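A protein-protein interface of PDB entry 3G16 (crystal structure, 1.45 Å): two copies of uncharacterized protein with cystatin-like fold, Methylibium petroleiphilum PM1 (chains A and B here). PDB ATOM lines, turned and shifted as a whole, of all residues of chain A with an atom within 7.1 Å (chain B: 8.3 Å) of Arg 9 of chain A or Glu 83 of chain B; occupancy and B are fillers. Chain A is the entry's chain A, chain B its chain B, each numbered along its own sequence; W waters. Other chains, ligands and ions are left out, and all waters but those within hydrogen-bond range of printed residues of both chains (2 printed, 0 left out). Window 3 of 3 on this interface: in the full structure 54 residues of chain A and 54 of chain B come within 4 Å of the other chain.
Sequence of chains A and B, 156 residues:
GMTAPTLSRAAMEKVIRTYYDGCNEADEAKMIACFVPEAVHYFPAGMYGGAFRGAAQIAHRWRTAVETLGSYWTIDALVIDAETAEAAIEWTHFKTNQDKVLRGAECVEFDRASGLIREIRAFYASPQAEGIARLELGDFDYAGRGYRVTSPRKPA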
ATOM      1  N   THR A   6      20.915  -9.955  -4.396  1.00  0.00           N
ATOM      2  CA  THR A   6      20.458 -10.249  -5.741  1.00  0.00           C
ATOM      3  C   THR A   6      21.123 -11.551  -6.165  1.00  0.00           C
ATOM      4  O   THR A   6      22.351 -11.621  -6.282  1.00  0.00           O
ATOM      5  CB  THR A   6      20.827  -9.132  -6.703  1.00  0.00           C
ATOM      6  OG1 THR A   6      20.108  -7.976  -6.305  1.00  0.00           O
ATOM      7  CG2 THR A   6      20.453  -9.489  -8.143  1.00  0.00           C
ATOM      8  N   LEU A   7      20.296 -12.557  -6.346  1.00  0.00           N
ATOM      9  CA  LEU A   7      20.762 -13.828  -6.884  1.00  0.00           C
ATOM     10  C   LEU A   7      20.897 -13.672  -8.396  1.00  0.00           C
ATOM     11  O   LEU A   7      20.032 -13.040  -9.038  1.00  0.00           O
ATOM     12  CB  LEU A   7      19.774 -14.950  -6.620  1.00  0.00           C
ATOM     13  CG  LEU A   7      19.501 -15.188  -5.153  1.00  0.00           C
ATOM     14  CD1 LEU A   7      18.484 -16.324  -4.969  1.00  0.00           C
ATOM     15  CD2 LEU A   7      20.776 -15.481  -4.323  1.00  0.00           C
ATOM     16  N   SER A   8      21.949 -14.232  -8.980  1.00  0.00           N
ATOM     17  CA  SER A   8      22.079 -14.215 -10.435  1.00  0.00           C
ATOM     18  C   SER A   8      21.052 -15.113 -11.088  1.00  0.00           C
ATOM     19  O   SER A   8      20.541 -16.075 -10.489  1.00  0.00           O
ATOM     20  CB  SER A   8      23.477 -14.668 -10.858  1.00  0.00           C
ATOM     21  OG  SER A   8      23.636 -16.050 -10.649  1.00  0.00           O
ATOM     22  N   ARG A   9      20.746 -14.838 -12.344  1.00  0.00           N
ATOM     23  CA  ARG A   9      19.820 -15.703 -13.064  1.00  0.00           C
ATOM     24  C   ARG A   9      20.401 -17.100 -13.168  1.00  0.00           C
ATOM     25  O   ARG A   9      19.691 -18.071 -12.993  1.00  0.00           O
ATOM     26  CB  ARG A   9      19.459 -15.173 -14.459  1.00  0.00           C
ATOM     27  CG  ARG A   9      20.517 -15.233 -15.545  1.00  0.00           C
ATOM     28  CD  ARG A   9      19.862 -15.004 -16.953  1.00  0.00           C
ATOM     29  NE  ARG A   9      18.701 -14.166 -16.741  1.00  0.00           N
ATOM     30  CZ  ARG A   9      17.437 -14.454 -17.022  1.00  0.00           C
ATOM     31  NH1 ARG A   9      17.082 -15.507 -17.768  1.00  0.00           N
ATOM     32  NH2 ARG A   9      16.546 -13.572 -16.641  1.00  0.00           N
ATOM     33  N   ALA A  10      21.694 -17.207 -13.441  1.00  0.00           N
ATOM     34  CA  ALA A  10      22.368 -18.504 -13.545  1.00  0.00           C
ATOM     35  C   ALA A  10      22.260 -19.314 -12.267  1.00  0.00           C
ATOM     36  O   ALA A  10      22.095 -20.522 -12.301  1.00  0.00           O
ATOM     37  CB  ALA A  10      23.839 -18.329 -13.919  1.00  0.00           C
ATOM     38  N   ALA A  11      22.418 -18.647 -11.128  1.00  0.00           N
ATOM     39  CA  ALA A  11      22.321 -19.344  -9.846  1.00  0.00           C
ATOM     40  C   ALA A  11      20.956 -19.948  -9.637  1.00  0.00           C
ATOM     41  O   ALA A  11      20.822 -21.047  -9.120  1.00  0.00           O
ATOM     42  CB  ALA A  11      22.667 -18.370  -8.743  1.00  0.00           C
ATOM     43  N   MET A  12      19.924 -19.204  -9.967  1.00  0.00           N
ATOM     44  CA  MET A  12      18.545 -19.699  -9.806  1.00  0.00           C
ATOM     45  C   MET A  12      18.267 -20.824 -10.772  1.00  0.00           C
ATOM     46  O   MET A  12      17.693 -21.850 -10.412  1.00  0.00           O
ATOM     47  CB  MET A  12      17.542 -18.549  -9.961  1.00  0.00           C
ATOM     48  CG  MET A  12      17.519 -17.674  -8.724  1.00  0.00           C
ATOM     49  SD  MET A  12      16.093 -16.344  -8.823  1.00  0.00           S
ATOM     50  CE  MET A  12      17.003 -15.207  -9.882  1.00  0.00           C
ATOM     51  N   GLU A  13      18.750 -20.678 -12.000  1.00  0.00           N
ATOM     52  CA  GLU A  13      18.546 -21.738 -12.980  1.00  0.00           C
ATOM     53  C   GLU A  13      19.223 -23.023 -12.531  1.00  0.00           C
ATOM     54  O   GLU A  13      18.665 -24.100 -12.691  1.00  0.00           O
ATOM     55  CB  GLU A  13      19.098 -21.336 -14.344  1.00  0.00           C
ATOM     56  CG  GLU A  13      18.859 -22.371 -15.375  1.00  0.00           C
ATOM     57  CD  GLU A  13      19.184 -21.925 -16.773  1.00  0.00           C
ATOM     58  OE1 GLU A  13      19.430 -20.706 -16.962  1.00  0.00           O
ATOM     59  OE2 GLU A  13      19.189 -22.798 -17.683  1.00  0.00           O
ATOM     60  N   LYS A  14      20.426 -22.921 -11.977  1.00  0.00           N
ATOM     61  CA  LYS A  14      21.174 -24.086 -11.530  1.00  0.00           C
ATOM     62  C   LYS A  14      20.437 -24.829 -10.437  1.00  0.00           C
ATOM     63  O   LYS A  14      20.357 -26.069 -10.468  1.00  0.00           O
ATOM     64  CB  LYS A  14      22.595 -23.703 -11.094  1.00  0.00           C
ATOM     65  CG  LYS A  14      23.475 -23.372 -12.288  1.00  0.00           C
ATOM     66  CD  LYS A  14      24.793 -22.715 -11.901  1.00  0.00           C
ATOM     67  CE  LYS A  14      25.483 -22.075 -13.094  1.00  0.00           C
ATOM     68  NZ  LYS A  14      26.439 -21.117 -12.729  1.00  0.00           N
ATOM     69  N   VAL A  15      19.894 -24.106  -9.449  1.00  0.00           N
ATOM     70  CA  VAL A  15      19.135 -24.788  -8.412  1.00  0.00           C
ATOM     71  C   VAL A  15      17.881 -25.469  -8.963  1.00  0.00           C
ATOM     72  O   VAL A  15      17.574 -26.625  -8.627  1.00  0.00           O
ATOM     73  CB  VAL A  15      18.745 -23.784  -7.316  1.00  0.00           C
ATOM     74  CG1 VAL A  15      17.791 -24.390  -6.278  1.00  0.00           C
ATOM     75  CG2 VAL A  15      20.008 -23.257  -6.606  1.00  0.00           C
ATOM     76  N   LEU A  78      11.133 -21.674 -18.804  1.00  0.00           N
ATOM     77  CA  LEU A  78      11.741 -21.230 -17.563  1.00  0.00           C
ATOM     78  C   LEU A  78      11.866 -19.712 -17.599  1.00  0.00           C
ATOM     79  O   LEU A  78      12.541 -19.174 -18.485  1.00  0.00           O
ATOM     80  CB  LEU A  78      13.101 -21.922 -17.388  1.00  0.00           C
ATOM     81  CG  LEU A  78      13.900 -21.568 -16.170  1.00  0.00           C
ATOM     82  CD1 LEU A  78      13.078 -21.697 -14.850  1.00  0.00           C
ATOM     83  CD2 LEU A  78      15.158 -22.468 -16.190  1.00  0.00           C
ATOM     84  N   VAL A  79      11.210 -19.018 -16.684  1.00  0.00           N
ATOM     85  CA  VAL A  79      11.167 -17.568 -16.621  1.00  0.00           C
ATOM     86  C   VAL A  79      11.847 -17.173 -15.322  1.00  0.00           C
ATOM     87  O   VAL A  79      11.439 -17.621 -14.265  1.00  0.00           O
ATOM     88  CB  VAL A  79       9.703 -17.084 -16.566  1.00  0.00           C
ATOM     89  CG1 VAL A  79       9.598 -15.574 -16.536  1.00  0.00           C
ATOM     90  CG2 VAL A  79       8.906 -17.638 -17.782  1.00  0.00           C
ATOM     91  N   ILE A  80      12.936 -16.424 -15.400  1.00  0.00           N
ATOM     92  CA  ILE A  80      13.721 -16.075 -14.224  1.00  0.00           C
ATOM     93  C   ILE A  80      13.811 -14.570 -14.039  1.00  0.00           C
ATOM     94  O   ILE A  80      14.180 -13.835 -14.960  1.00  0.00           O
ATOM     95  CB  ILE A  80      15.135 -16.712 -14.254  1.00  0.00           C
ATOM     96  CG1 ILE A  80      15.030 -18.231 -14.343  1.00  0.00           C
ATOM     97  CG2 ILE A  80      15.937 -16.236 -13.003  1.00  0.00           C
ATOM     98  CD1 ILE A  80      16.353 -18.877 -14.703  1.00  0.00           C
ATOM     99  N   ASP A  81      13.450 -14.128 -12.839  1.00  0.00           N
ATOM    100  CA  ASP A  81      13.380 -12.690 -12.506  1.00  0.00           C
ATOM    101  C   ASP A  81      14.406 -12.356 -11.402  1.00  0.00           C
ATOM    102  O   ASP A  81      14.162 -12.574 -10.201  1.00  0.00           O
ATOM    103  CB  ASP A  81      11.953 -12.333 -12.086  1.00  0.00           C
ATOM    104  CG  ASP A  81      11.709 -10.847 -11.944  1.00  0.00           C
ATOM    105  OD1 ASP A  81      12.654 -10.070 -11.734  1.00  0.00           O
ATOM    106  OD2 ASP A  81      10.540 -10.456 -12.033  1.00  0.00           O
ATOM    107  N   ALA A  82      15.551 -11.790 -11.815  1.00  0.00           N
ATOM    108  CA  ALA A  82      16.557 -11.418 -10.823  1.00  0.00           C
ATOM    109  C   ALA A  82      16.162 -10.198  -9.980  1.00  0.00           C
ATOM    110  O   ALA A  82      16.745  -9.964  -8.941  1.00  0.00           O
ATOM    111  CB  ALA A  82      17.898 -11.192 -11.480  1.00  0.00           C
ATOM    112  N   PRO B   5      15.385  -7.226 -30.639  1.00  0.00           N
ATOM    113  CA  PRO B   5      15.597  -6.004 -29.847  1.00  0.00           C
ATOM    114  C   PRO B   5      15.335  -6.185 -28.340  1.00  0.00           C
ATOM    115  O   PRO B   5      14.620  -7.113 -27.926  1.00  0.00           O
ATOM    116  CB  PRO B   5      14.609  -4.989 -30.457  1.00  0.00           C
ATOM    117  CG  PRO B   5      13.777  -5.750 -31.458  1.00  0.00           C
ATOM    118  CD  PRO B   5      14.529  -6.995 -31.816  1.00  0.00           C
ATOM    119  N   THR B   6      15.911  -5.289 -27.536  1.00  0.00           N
ATOM    120  CA  THR B   6      15.771  -5.350 -26.072  1.00  0.00           C
ATOM    121  C   THR B   6      14.433  -4.793 -25.591  1.00  0.00           C
ATOM    122  O   THR B   6      13.869  -3.851 -26.151  1.00  0.00           O
ATOM    123  CB  THR B   6      16.934  -4.629 -25.335  1.00  0.00           C
ATOM    124  OG1 THR B   6      18.148  -5.362 -25.551  1.00  0.00           O
ATOM    125  CG2 THR B   6      16.677  -4.545 -23.817  1.00  0.00           C
ATOM    126  N   LEU B   7      13.953  -5.400 -24.532  1.00  0.00           N
ATOM    127  CA  LEU B   7      12.687  -5.060 -23.953  1.00  0.00           C
ATOM    128  C   LEU B   7      12.985  -5.078 -22.465  1.00  0.00           C
ATOM    129  O   LEU B   7      13.501  -6.057 -21.951  1.00  0.00           O
ATOM    130  CB  LEU B   7      11.689  -6.118 -24.410  1.00  0.00           C
ATOM    131  CG  LEU B   7      10.246  -6.104 -23.965  1.00  0.00           C
ATOM    132  CD1 LEU B   7       9.572  -4.719 -24.130  1.00  0.00           C
ATOM    133  CD2 LEU B   7       9.510  -7.194 -24.749  1.00  0.00           C
ATOM    134  N   SER B   8      12.738  -3.972 -21.787  1.00  0.00           N
ATOM    135  CA  SER B   8      13.038  -3.891 -20.368  1.00  0.00           C
ATOM    136  C   SER B   8      11.966  -4.560 -19.495  1.00  0.00           C
ATOM    137  O   SER B   8      10.806  -4.715 -19.903  1.00  0.00           O
ATOM    138  CB  SER B   8      13.171  -2.438 -19.921  1.00  0.00           C
ATOM    139  OG  SER B   8      11.925  -1.762 -19.844  1.00  0.00           O
ATOM    140  N   ARG B   9      12.370  -4.927 -18.289  1.00  0.00           N
ATOM    141  CA  ARG B   9      11.444  -5.477 -17.318  1.00  0.00           C
ATOM    142  C   ARG B   9      10.297  -4.472 -17.063  1.00  0.00           C
ATOM    143  O   ARG B   9       9.121  -4.858 -17.026  1.00  0.00           O
ATOM    144  CB  ARG B   9      12.162  -5.797 -15.991  1.00  0.00           C
ATOM    145  CG  ARG B   9      11.343  -6.663 -15.040  1.00  0.00           C
ATOM    146  CD  ARG B   9      11.955  -6.716 -13.589  1.00  0.00           C
ATOM    147  NE  ARG B   9      11.106  -7.563 -12.808  1.00  0.00           N
ATOM    148  CZ  ARG B   9       9.941  -7.207 -12.285  1.00  0.00           C
ATOM    149  NH1 ARG B   9       9.489  -5.961 -12.439  1.00  0.00           N
ATOM    150  NH2 ARG B   9       9.178  -8.068 -11.643  1.00  0.00           N
ATOM    151  N   MET B  12       7.754  -4.407 -19.932  1.00  0.00           N
ATOM    152  CA  MET B  12       6.870  -5.589 -19.898  1.00  0.00           C
ATOM    153  C   MET B  12       5.846  -5.446 -18.792  1.00  0.00           C
ATOM    154  O   MET B  12       4.647  -5.760 -18.984  1.00  0.00           O
ATOM    155  CB  MET B  12       7.635  -6.909 -19.758  1.00  0.00           C
ATOM    156  CG  MET B  12       8.200  -7.396 -21.087  1.00  0.00           C
ATOM    157  SD  MET B  12       9.133  -9.049 -20.989  1.00  0.00           S
ATOM    158  CE  MET B  12      10.839  -8.265 -20.214  1.00  0.00           C
ATOM    159  N   ILE B  80       9.086 -11.510 -14.229  1.00  0.00           N
ATOM    160  CA  ILE B  80       9.391 -10.979 -15.551  1.00  0.00           C
ATOM    161  C   ILE B  80      10.858 -11.234 -15.877  1.00  0.00           C
ATOM    162  O   ILE B  80      11.749 -10.855 -15.106  1.00  0.00           O
ATOM    163  CB  ILE B  80       9.085  -9.465 -15.634  1.00  0.00           C
ATOM    164  CG1 ILE B  80       7.606  -9.196 -15.300  1.00  0.00           C
ATOM    165  CG2 ILE B  80       9.521  -8.900 -16.988  1.00  0.00           C
ATOM    166  CD1 ILE B  80       7.267  -7.751 -15.234  1.00  0.00           C
ATOM    167  N   ASP B  81      11.099 -11.854 -17.028  1.00  0.00           N
ATOM    168  CA  ASP B  81      12.442 -12.203 -17.487  1.00  0.00           C
ATOM    169  C   ASP B  81      12.837 -11.331 -18.675  1.00  0.00           C
ATOM    170  O   ASP B  81      12.448 -11.612 -19.815  1.00  0.00           O
ATOM    171  CB  ASP B  81      12.480 -13.675 -17.860  1.00  0.00           C
ATOM    172  CG  ASP B  81      13.882 -14.209 -18.041  1.00  0.00           C
ATOM    173  OD1 ASP B  81      14.773 -13.408 -18.440  1.00  0.00           O
ATOM    174  OD2 ASP B  81      14.083 -15.427 -17.815  1.00  0.00           O
ATOM    175  N   ALA B  82      13.650 -10.316 -18.406  1.00  0.00           N
ATOM    176  CA  ALA B  82      14.077  -9.382 -19.433  1.00  0.00           C
ATOM    177  C   ALA B  82      15.070 -10.009 -20.391  1.00  0.00           C
ATOM    178  O   ALA B  82      15.240  -9.476 -21.495  1.00  0.00           O
ATOM    179  CB  ALA B  82      14.634  -8.088 -18.817  1.00  0.00           C
ATOM    180  N   GLU B  83      15.725 -11.093 -20.009  1.00  0.00           N
ATOM    181  CA  GLU B  83      16.656 -11.788 -20.894  1.00  0.00           C
ATOM    182  C   GLU B  83      15.897 -12.552 -21.997  1.00  0.00           C
ATOM    183  O   GLU B  83      16.311 -12.597 -23.138  1.00  0.00           O
ATOM    184  CB  GLU B  83      17.528 -12.759 -20.077  1.00  0.00           C
ATOM    185  CG  GLU B  83      18.523 -13.614 -20.862  1.00  0.00           C
ATOM    186  CD  GLU B  83      19.689 -12.838 -21.427  1.00  0.00           C
ATOM    187  OE1 GLU B  83      20.011 -11.743 -20.918  1.00  0.00           O
ATOM    188  OE2 GLU B  83      20.307 -13.343 -22.391  1.00  0.00           O
ATOM    189  N   THR B  84      14.767 -13.149 -21.664  1.00  0.00           N
ATOM    190  CA  THR B  84      14.029 -13.955 -22.636  1.00  0.00           C
ATOM    191  C   THR B  84      12.759 -13.295 -23.164  1.00  0.00           C
ATOM    192  O   THR B  84      12.049 -13.868 -23.980  1.00  0.00           O
ATOM    193  CB  THR B  84      13.635 -15.290 -21.976  1.00  0.00           C
ATOM    194  OG1 THR B  84      12.724 -15.025 -20.896  1.00  0.00           O
ATOM    195  CG2 THR B  84      14.839 -16.051 -21.427  1.00  0.00           C
ATOM    196  N   ALA B  85      12.428 -12.120 -22.666  1.00  0.00           N
ATOM    197  CA  ALA B  85      11.202 -11.449 -23.075  1.00  0.00           C
ATOM    198  C   ALA B  85       9.971 -12.311 -22.797  1.00  0.00           C
ATOM    199  O   ALA B  85       9.054 -12.436 -23.622  1.00  0.00           O
ATOM    200  CB  ALA B  85      11.252 -11.033 -24.578  1.00  0.00           C
ATOM    201  N   GLU B  86       9.965 -12.908 -21.599  1.00  0.00           N
ATOM    202  CA  GLU B  86       8.858 -13.722 -21.154  1.00  0.00           C
ATOM    203  C   GLU B  86       8.508 -13.308 -19.734  1.00  0.00           C
ATOM    204  O   GLU B  86       9.330 -12.755 -18.997  1.00  0.00           O
ATOM    205  CB  GLU B  86       9.189 -15.227 -21.195  1.00  0.00           C
ATOM    206  CG  GLU B  86       9.411 -15.753 -22.636  1.00  0.00           C
ATOM    207  CD  GLU B  86       9.575 -17.273 -22.770  1.00  0.00           C
ATOM    208  OE1 GLU B  86       9.827 -17.996 -21.793  1.00  0.00           O
ATOM    209  OE2 GLU B  86       9.515 -17.756 -23.933  1.00  0.00           O
ATOM    210  N   ARG B 112       9.402  -9.040 -29.330  1.00  0.00           N
ATOM    211  CA  ARG B 112      10.419  -8.011 -29.043  1.00  0.00           C
ATOM    212  C   ARG B 112      10.349  -6.758 -29.892  1.00  0.00           C
ATOM    213  O   ARG B 112      10.561  -5.661 -29.394  1.00  0.00           O
ATOM    214  CB  ARG B 112      11.819  -8.593 -29.182  1.00  0.00           C
ATOM    215  CG  ARG B 112      12.150  -9.591 -28.129  1.00  0.00           C
ATOM    216  CD  ARG B 112      13.437 -10.302 -28.508  1.00  0.00           C
ATOM    217  NE  ARG B 112      13.810 -11.337 -27.548  1.00  0.00           N
ATOM    218  CZ  ARG B 112      14.451 -11.105 -26.411  1.00  0.00           C
ATOM    219  NH1 ARG B 112      14.771  -9.866 -26.037  1.00  0.00           N
ATOM    220  NH2 ARG B 112      14.751 -12.133 -25.631  1.00  0.00           N
HETATM  221  O   HOH W   1      11.693 -17.216 -20.148  1.00  0.00           O
HETATM  222  O   HOH W   2      11.259 -20.330 -21.581  1.00  0.00           O
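Arg 9 of chain A touches Asp 81 of chain B, and with the chains exchanged Asp 81 of chain A touches Arg 9 of chain B. Ile 80 of chain A touches its own counterpart, Ile 80 of chain B. Ile 80 of chain A touches Asp 81 of chain B, and with the chains exchanged Asp 81 of chain A touches Ile 80 of chain B. Of the 8 pairs that touch across the chains among the printed residues, 5 have their exchanged pair printed and touching as well.
NH2 of Arg 9 of chain A lies within salt-bridge range of OD1 of Asp 81 of chain B. The backbone NH (N) of Ile 80 of chain A is in hydrogen-bond range of the side-chain carboxylate (OD2) of Asp 81 of chain B (2.9 Å). The side-chain carboxylate (OD2) of Asp 81 of chain A lies within salt-bridge range of the guanidinium group (NH2) of Arg 9 of chain B (2.8 Å). N of Ile 80 of chain B sits at hydrogen-bond distance from OD2 of Asp 81 of chain A, at 2.8 Å.
Ala 10 of chain A touches none of the printed residues of chain B. Of the printed residues of chain B, Val 79 of chain A touches Asp 81 and Glu 86. Ala 82 of chain A touches none of the printed residues of chain B. Printed residues of chain A within 4 Å of Arg 9 of chain B: Asp 81. Of the printed residues of chain A, Ile 80 of chain B touches Ile 80 (3.8 Å) and Asp 81 (2.8 Å). Of the printed residues of chain A, Glu 83 of chain B touches Arg 9 (3.5 Å). The nearest printed residue of chain A that does not touch Glu 83 of chain B is Ile 80 of chain A (5.9 Å). The nearest printed residue of chain A that does not touch Ile 80 of chain B is Val 79 of chain A (4.6 Å).
Among the printed residues, pairs that only touch across the chains: Arg 9 of chain A with Glu 83 of chain B (3.5 Å), Val 79 of chain A with Asp 81 of chain B (3.7 Å), Val 79 of chain A with Glu 86 of chain B (3.8 Å) and Ile 80 of chain A with Ile 80 of chain B (3.8 Å).
Water W1 lies within hydrogen-bond range of OG1 of Thr 84 of chain B (2.5 Å), OE1 of Glu 86 of chain B (2.6 Å) and O of Leu 78 of chain A (2.7 Å). Water W2 lies within hydrogen-bond range of OE1 of Glu 86 of chain B and N of Leu 78 of chain A.
Of the 14 printed residues of chain B, 5 touch a printed residue of chain A. Printed residues of chain B that touch a printed residue of chain A: Arg 9, Ile 80, Asp 81, Glu 83 and Glu 86. Along chain B the printed residues that touch a printed residue of chain A span positions 9 to 86.
NH2 of Arg 9 of chain A is in hydrogen-bond range of O of Ile 80 of chain A (2.9 Å). OD1 of Asp 81 of chain B lies within hydrogen-bond range of N of Glu 83 of chain B (3.0 Å). OD1 of Asp 81 of chain B sits at hydrogen-bond distance from N of Thr 84 of chain B (3.2 Å). The backbone NH (N) of Asp 81 of chain B is in hydrogen-bond range of the backbone carbonyl oxygen (O) of Glu 86 of chain B (2.8 Å). The backbone carbonyl oxygen (O) of Glu 83 of chain B sits at hydrogen-bond distance from the guanidinium group (NH2) of Arg 112 of chain B.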
